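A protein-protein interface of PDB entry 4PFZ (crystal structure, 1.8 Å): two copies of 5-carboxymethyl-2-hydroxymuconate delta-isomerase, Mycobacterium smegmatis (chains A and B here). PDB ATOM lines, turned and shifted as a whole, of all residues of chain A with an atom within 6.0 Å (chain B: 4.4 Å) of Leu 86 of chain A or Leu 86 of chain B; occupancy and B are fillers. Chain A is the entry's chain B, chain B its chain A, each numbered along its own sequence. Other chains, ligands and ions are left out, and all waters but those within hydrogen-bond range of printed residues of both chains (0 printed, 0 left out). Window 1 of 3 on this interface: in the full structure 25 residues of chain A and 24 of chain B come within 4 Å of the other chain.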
ATOM      1  N   LYS A  59      21.973 -10.142  -8.515  1.00  0.00           N
ATOM      2  CA  LYS A  59      21.030 -10.576  -7.490  1.00  0.00           C
ATOM      3  C   LYS A  59      19.600 -10.216  -7.863  1.00  0.00           C
ATOM      4  O   LYS A  59      19.354  -9.319  -8.680  1.00  0.00           O
ATOM      5  CB  LYS A  59      21.379  -9.983  -6.115  1.00  0.00           C
ATOM      6  CG  LYS A  59      21.484  -8.463  -6.042  1.00  0.00           C
ATOM      7  CD  LYS A  59      21.893  -8.031  -4.612  1.00  0.00           C
ATOM      8  CE  LYS A  59      22.347  -6.571  -4.534  1.00  0.00           C
ATOM      9  NZ  LYS A  59      23.349  -6.224  -5.578  1.00  0.00           N
ATOM     10  N   VAL A  60      18.671 -10.932  -7.251  1.00  0.00           N
ATOM     11  CA  VAL A  60      17.273 -10.708  -7.471  1.00  0.00           C
ATOM     12  C   VAL A  60      16.663 -10.470  -6.115  1.00  0.00           C
ATOM     13  O   VAL A  60      16.714 -11.354  -5.263  1.00  0.00           O
ATOM     14  CB  VAL A  60      16.594 -11.910  -8.137  1.00  0.00           C
ATOM     15  CG1 VAL A  60      15.072 -11.674  -8.231  1.00  0.00           C
ATOM     16  CG2 VAL A  60      17.191 -12.164  -9.500  1.00  0.00           C
ATOM     17  N   ILE A  61      16.076  -9.287  -5.930  1.00  0.00           N
ATOM     18  CA  ILE A  61      15.368  -8.945  -4.705  1.00  0.00           C
ATOM     19  C   ILE A  61      13.878  -9.057  -4.969  1.00  0.00           C
ATOM     20  O   ILE A  61      13.394  -8.632  -6.022  1.00  0.00           O
ATOM     21  CB  ILE A  61      15.687  -7.505  -4.225  1.00  0.00           C
ATOM     22  CG1 ILE A  61      17.155  -7.405  -3.843  1.00  0.00           C
ATOM     23  CG2 ILE A  61      14.859  -7.137  -3.003  1.00  0.00           C
ATOM     24  CD1 ILE A  61      18.071  -7.021  -4.990  1.00  0.00           C
ATOM     25  N   ALA A  62      13.145  -9.621  -4.028  1.00  0.00           N
ATOM     26  CA  ALA A  62      11.708  -9.683  -4.212  1.00  0.00           C
ATOM     27  C   ALA A  62      10.974  -9.257  -2.958  1.00  0.00           C
ATOM     28  O   ALA A  62      11.522  -9.296  -1.864  1.00  0.00           O
ATOM     29  CB  ALA A  62      11.298 -11.093  -4.624  1.00  0.00           C
ATOM     30  N   ILE A  84      11.585  -7.597   2.353  1.00  0.00           N
ATOM     31  CA  ILE A  84      12.299  -7.991   1.142  1.00  0.00           C
ATOM     32  C   ILE A  84      13.126  -9.255   1.379  1.00  0.00           C
ATOM     33  O   ILE A  84      13.459  -9.589   2.517  1.00  0.00           O
ATOM     34  CB  ILE A  84      13.200  -6.846   0.609  1.00  0.00           C
ATOM     35  CG1 ILE A  84      14.193  -6.388   1.674  1.00  0.00           C
ATOM     36  CG2 ILE A  84      12.340  -5.671   0.114  1.00  0.00           C
ATOM     37  CD1 ILE A  84      15.262  -5.443   1.153  1.00  0.00           C
ATOM     38  N   PHE A  85      13.408  -9.979   0.303  1.00  0.00           N
ATOM     39  CA  PHE A  85      14.238 -11.184   0.368  1.00  0.00           C
ATOM     40  C   PHE A  85      14.980 -11.390  -0.966  1.00  0.00           C
ATOM     41  O   PHE A  85      14.833 -10.599  -1.896  1.00  0.00           O
ATOM     42  CB  PHE A  85      13.393 -12.425   0.721  1.00  0.00           C
ATOM     43  CG  PHE A  85      12.245 -12.684  -0.238  1.00  0.00           C
ATOM     44  CD1 PHE A  85      11.027 -12.061  -0.066  1.00  0.00           C
ATOM     45  CD2 PHE A  85      12.396 -13.554  -1.303  1.00  0.00           C
ATOM     46  CE1 PHE A  85       9.966 -12.292  -0.944  1.00  0.00           C
ATOM     47  CE2 PHE A  85      11.345 -13.783  -2.185  1.00  0.00           C
ATOM     48  CZ  PHE A  85      10.131 -13.157  -2.000  1.00  0.00           C
ATOM     49  N   LEU A  86      15.798 -12.439  -1.039  1.00  0.00           N
ATOM     50  CA  LEU A  86      16.647 -12.682  -2.203  1.00  0.00           C
ATOM     51  C   LEU A  86      16.287 -14.003  -2.885  1.00  0.00           C
ATOM     52  O   LEU A  86      15.951 -14.972  -2.217  1.00  0.00           O
ATOM     53  CB  LEU A  86      18.132 -12.720  -1.795  1.00  0.00           C
ATOM     54  CG  LEU A  86      18.757 -11.384  -1.412  1.00  0.00           C
ATOM     55  CD1 LEU A  86      20.135 -11.612  -0.798  1.00  0.00           C
ATOM     56  CD2 LEU A  86      18.847 -10.462  -2.636  1.00  0.00           C
ATOM     57  N   LYS A  87      16.352 -14.015  -4.211  1.00  0.00           N
ATOM     58  CA  LYS A  87      16.343 -15.258  -4.991  1.00  0.00           C
ATOM     59  C   LYS A  87      17.712 -15.341  -5.643  1.00  0.00           C
ATOM     60  O   LYS A  87      18.247 -14.325  -6.075  1.00  0.00           O
ATOM     61  CB  LYS A  87      15.206 -15.261  -6.023  1.00  0.00           C
ATOM     62  CG  LYS A  87      13.814 -15.282  -5.401  1.00  0.00           C
ATOM     63  CD  LYS A  87      12.687 -15.036  -6.438  1.00  0.00           C
ATOM     64  CE  LYS A  87      12.549 -16.147  -7.488  1.00  0.00           C
ATOM     65  NZ  LYS A  87      11.677 -17.284  -7.042  1.00  0.00           N
ATOM     66  N   PRO A  88      18.337 -16.533  -5.645  1.00  0.00           N
ATOM     67  CA  PRO A  88      19.646 -16.627  -6.288  1.00  0.00           C
ATOM     68  C   PRO A  88      19.570 -16.449  -7.788  1.00  0.00           C
ATOM     69  O   PRO A  88      18.591 -16.869  -8.386  1.00  0.00           O
ATOM     70  CB  PRO A  88      20.106 -18.049  -5.943  1.00  0.00           C
ATOM     71  CG  PRO A  88      18.819 -18.839  -5.845  1.00  0.00           C
ATOM     72  CD  PRO A  88      17.798 -17.856  -5.270  1.00  0.00           C
ATOM     73  N   MET A 156      13.703 -18.539   1.346  1.00  0.00           N
ATOM     74  CA  MET A 156      14.748 -18.611   0.331  1.00  0.00           C
ATOM     75  C   MET A 156      14.750 -19.965  -0.406  1.00  0.00           C
ATOM     76  O   MET A 156      14.713 -19.980  -1.630  1.00  0.00           O
ATOM     77  CB  MET A 156      16.130 -18.353   0.952  1.00  0.00           C
ATOM     78  CG  MET A 156      17.221 -18.044  -0.085  1.00  0.00           C
ATOM     79  SD  MET A 156      17.880 -19.507  -0.931  1.00  0.00           S
ATOM     80  CE  MET A 156      19.034 -20.092   0.295  1.00  0.00           C
ATOM     81  N   LYS A 159      11.955 -20.571  -2.817  1.00  0.00           N
ATOM     82  CA  LYS A 159      11.909 -19.712  -3.982  1.00  0.00           C
ATOM     83  C   LYS A 159      13.222 -19.725  -4.742  1.00  0.00           C
ATOM     84  O   LYS A 159      13.383 -18.975  -5.710  1.00  0.00           O
ATOM     85  CB  LYS A 159      11.556 -18.283  -3.563  1.00  0.00           C
ATOM     86  CG  LYS A 159      10.183 -18.141  -2.922  1.00  0.00           C
ATOM     87  CD  LYS A 159      10.045 -16.788  -2.267  1.00  0.00           C
ATOM     88  CE  LYS A 159       8.641 -16.508  -1.762  1.00  0.00           C
ATOM     89  NZ  LYS A 159       7.678 -16.307  -2.876  1.00  0.00           N
ATOM     90  N   MET A 214      21.082  -2.238   0.820  1.00  0.00           N
ATOM     91  CA  MET A 214      22.184  -2.816   0.056  1.00  0.00           C
ATOM     92  C   MET A 214      22.472  -2.044  -1.228  1.00  0.00           C
ATOM     93  O   MET A 214      21.576  -1.449  -1.821  1.00  0.00           O
ATOM     94  CB  MET A 214      21.873  -4.278  -0.285  1.00  0.00           C
ATOM     95  CG  MET A 214      20.726  -4.437  -1.282  1.00  0.00           C
ATOM     96  SD  MET A 214      20.339  -6.186  -1.509  1.00  0.00           S
ATOM     97  CE  MET A 214      19.495  -6.557   0.016  1.00  0.00           C
ATOM     98  N   VAL B  60      26.254 -15.941  -1.428  1.00  0.00           N
ATOM     99  CA  VAL B  60      26.620 -16.356  -0.093  1.00  0.00           C
ATOM    100  C   VAL B  60      25.422 -17.020   0.572  1.00  0.00           C
ATOM    101  O   VAL B  60      24.402 -16.376   0.827  1.00  0.00           O
ATOM    102  CB  VAL B  60      27.073 -15.170   0.760  1.00  0.00           C
ATOM    103  CG1 VAL B  60      27.220 -15.594   2.198  1.00  0.00           C
ATOM    104  CG2 VAL B  60      28.384 -14.590   0.208  1.00  0.00           C
ATOM    105  N   ILE B  61      25.551 -18.304   0.859  1.00  0.00           N
ATOM    106  CA  ILE B  61      24.511 -19.049   1.551  1.00  0.00           C
ATOM    107  C   ILE B  61      24.879 -19.182   3.010  1.00  0.00           C
ATOM    108  O   ILE B  61      26.051 -19.304   3.340  1.00  0.00           O
ATOM    109  CB  ILE B  61      24.310 -20.458   0.943  1.00  0.00           C
ATOM    110  CG1 ILE B  61      23.958 -20.347  -0.553  1.00  0.00           C
ATOM    111  CG2 ILE B  61      23.191 -21.208   1.648  1.00  0.00           C
ATOM    112  CD1 ILE B  61      25.141 -20.303  -1.488  1.00  0.00           C
ATOM    113  N   PHE B  85      19.545 -19.514   3.963  1.00  0.00           N
ATOM    114  CA  PHE B  85      19.136 -18.216   3.440  1.00  0.00           C
ATOM    115  C   PHE B  85      20.320 -17.586   2.719  1.00  0.00           C
ATOM    116  O   PHE B  85      21.420 -18.144   2.691  1.00  0.00           O
ATOM    117  CB  PHE B  85      18.632 -17.310   4.568  1.00  0.00           C
ATOM    118  CG  PHE B  85      19.665 -17.050   5.639  1.00  0.00           C
ATOM    119  CD1 PHE B  85      19.810 -17.922   6.704  1.00  0.00           C
ATOM    120  CD2 PHE B  85      20.493 -15.939   5.569  1.00  0.00           C
ATOM    121  CE1 PHE B  85      20.765 -17.692   7.690  1.00  0.00           C
ATOM    122  CE2 PHE B  85      21.452 -15.713   6.546  1.00  0.00           C
ATOM    123  CZ  PHE B  85      21.583 -16.589   7.604  1.00  0.00           C
ATOM    124  N   LEU B  86      20.090 -16.421   2.131  1.00  0.00           N
ATOM    125  CA  LEU B  86      21.106 -15.754   1.343  1.00  0.00           C
ATOM    126  C   LEU B  86      21.540 -14.440   1.957  1.00  0.00           C
ATOM    127  O   LEU B  86      20.724 -13.717   2.542  1.00  0.00           O
ATOM    128  CB  LEU B  86      20.591 -15.463  -0.070  1.00  0.00           C
ATOM    129  CG  LEU B  86      20.409 -16.631  -1.031  1.00  0.00           C
ATOM    130  CD1 LEU B  86      19.750 -16.137  -2.317  1.00  0.00           C
ATOM    131  CD2 LEU B  86      21.760 -17.244  -1.342  1.00  0.00           C
ATOM    132  N   LYS B  87      22.814 -14.125   1.785  1.00  0.00           N
ATOM    133  CA  LYS B  87      23.298 -12.765   2.005  1.00  0.00           C
ATOM    134  C   LYS B  87      23.779 -12.271   0.654  1.00  0.00           C
ATOM    135  O   LYS B  87      24.364 -13.027  -0.102  1.00  0.00           O
ATOM    136  CB  LYS B  87      24.418 -12.739   3.060  1.00  0.00           C
ATOM    137  CG  LYS B  87      23.967 -13.157   4.456  1.00  0.00           C
ATOM    138  CD  LYS B  87      25.146 -13.418   5.416  1.00  0.00           C
ATOM    139  CE  LYS B  87      25.950 -12.142   5.732  1.00  0.00           C
ATOM    140  NZ  LYS B  87      25.379 -11.341   6.870  1.00  0.00           N
ATOM    141  N   PRO B  88      23.497 -10.995   0.310  1.00  0.00           N
ATOM    142  CA  PRO B  88      23.903 -10.502  -1.011  1.00  0.00           C
ATOM    143  C   PRO B  88      25.409 -10.377  -1.048  1.00  0.00           C
ATOM    144  O   PRO B  88      25.972 -10.102   0.021  1.00  0.00           O
ATOM    145  CB  PRO B  88      23.232  -9.122  -1.093  1.00  0.00           C
ATOM    146  CG  PRO B  88      23.210  -8.652   0.326  1.00  0.00           C
ATOM    147  CD  PRO B  88      22.995  -9.920   1.175  1.00  0.00           C
ATOM    148  N   MET B 156      16.747 -11.789   5.663  1.00  0.00           N
ATOM    149  CA  MET B 156      17.596 -11.207   4.637  1.00  0.00           C
ATOM    150  C   MET B 156      18.051  -9.753   4.922  1.00  0.00           C
ATOM    151  O   MET B 156      19.246  -9.473   4.937  1.00  0.00           O
ATOM    152  CB  MET B 156      16.882 -11.276   3.279  1.00  0.00           C
ATOM    153  CG  MET B 156      17.837 -11.143   2.085  1.00  0.00           C
ATOM    154  SD  MET B 156      18.377  -9.423   1.835  1.00  0.00           S
ATOM    155  CE  MET B 156      16.865  -8.723   1.201  1.00  0.00           C
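The backbone carbonyl oxygen of Val 60 of chain B lies within hydrogen-bond range of the backbone NH of Lys 87 of chain B (2.9 Å).
O of Val 60 of chain A is in hydrogen-bond range of N of Lys 87 of chain A.
N of Ala 62 of chain A sits at hydrogen-bond distance from O of Phe 85 of chain A (2.9 Å).
The backbone carbonyl oxygen (O) of Lys 159 of chain A is in hydrogen-bond range of the side-chain amino group (NZ) of Lys 87 of chain A (2.7 Å).
Among the printed residues, pairs that only touch across the chains: Met 214 of chain A with Met 156 of chain B, Ile 84 of chain A with Met 156 of chain B, Leu 86 of chain A with Pro 88 of chain B, Met 156 of chain A with Leu 86 of chain B, Leu 86 of chain A with Met 156 of chain B, Pro 88 of chain A with Leu 86 of chain B, Met 156 of chain A with Phe 85 of chain B, Phe 85 of chain A with Met 156 of chain B, Leu 86 of chain A with Leu 86 of chain B, Lys 59 of chain A with Pro 88 of chain B, Leu 86 of chain A with Lys 87 of chain B and Lys 87 of chain A with Leu 86 of chain B.
Of the printed residues of chain B, Leu 86 of chain A touches Leu 86, Lys 87, Pro 88 and Met 156.
Of the printed residues of chain A, Leu 86 of chain B touches Leu 86 (3.8 Å), Lys 87 (3.98 Å), Pro 88 (3.6 Å) and Met 156 (3.6 Å).
Of the printed residues of chain A, Phe 85 of chain B touches Met 156.
Printed residues of chain B within 4 Å of Lys 59 of chain A: Pro 88.
Ala 62 of chain A touches none of the printed residues of chain B.
Val 60 of chain B touches none of the printed residues of chain A.
The nearest printed residue of chain A that does not touch Leu 86 of chain B is Val 60 of chain A (6.4 Å).
Of the 12 printed residues of chain A, 8 touch a printed residue of chain B.
Printed residues of chain A that touch a printed residue of chain B: Lys 59, Ile 84, Phe 85, Leu 86, Lys 87, Pro 88, Met 156 and Met 214.
Hydrophobic or aromatic side chains of chain A within 4 Å of the printed part of chain B: Ile 84, Leu 86, Pro 88, Met 156 and Met 214.
Of the 7 printed residues of chain B, 5 touch a printed residue of chain A.
Among the printed residues, 12 pairs touch across the chains.
Among the printed residues, no Asp or Glu carboxylate lies within 4 Å of a Lys or Arg side-chain nitrogen of the other chain.
Phe 85 of chain A touches Met 156 of chain B, and with the chains exchanged Met 156 of chain A touches Phe 85 of chain B.
Leu 86 of chain A touches its own counterpart, Leu 86 of chain B.
Leu 86 of chain A touches Pro 88 of chain B, and with the chains exchanged Pro 88 of chain A touches Leu 86 of chain B.
Leu 86 of chain A touches Met 156 of chain B, and with the chains exchanged Met 156 of chain A touches Leu 86 of chain B.
Positions printed for both chains: 60, 61, 85, 86, 87, 88 and 156.
Of the 12 pairs that touch across the chains among the printed residues, 9 have their exchanged pair printed and touching as well.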
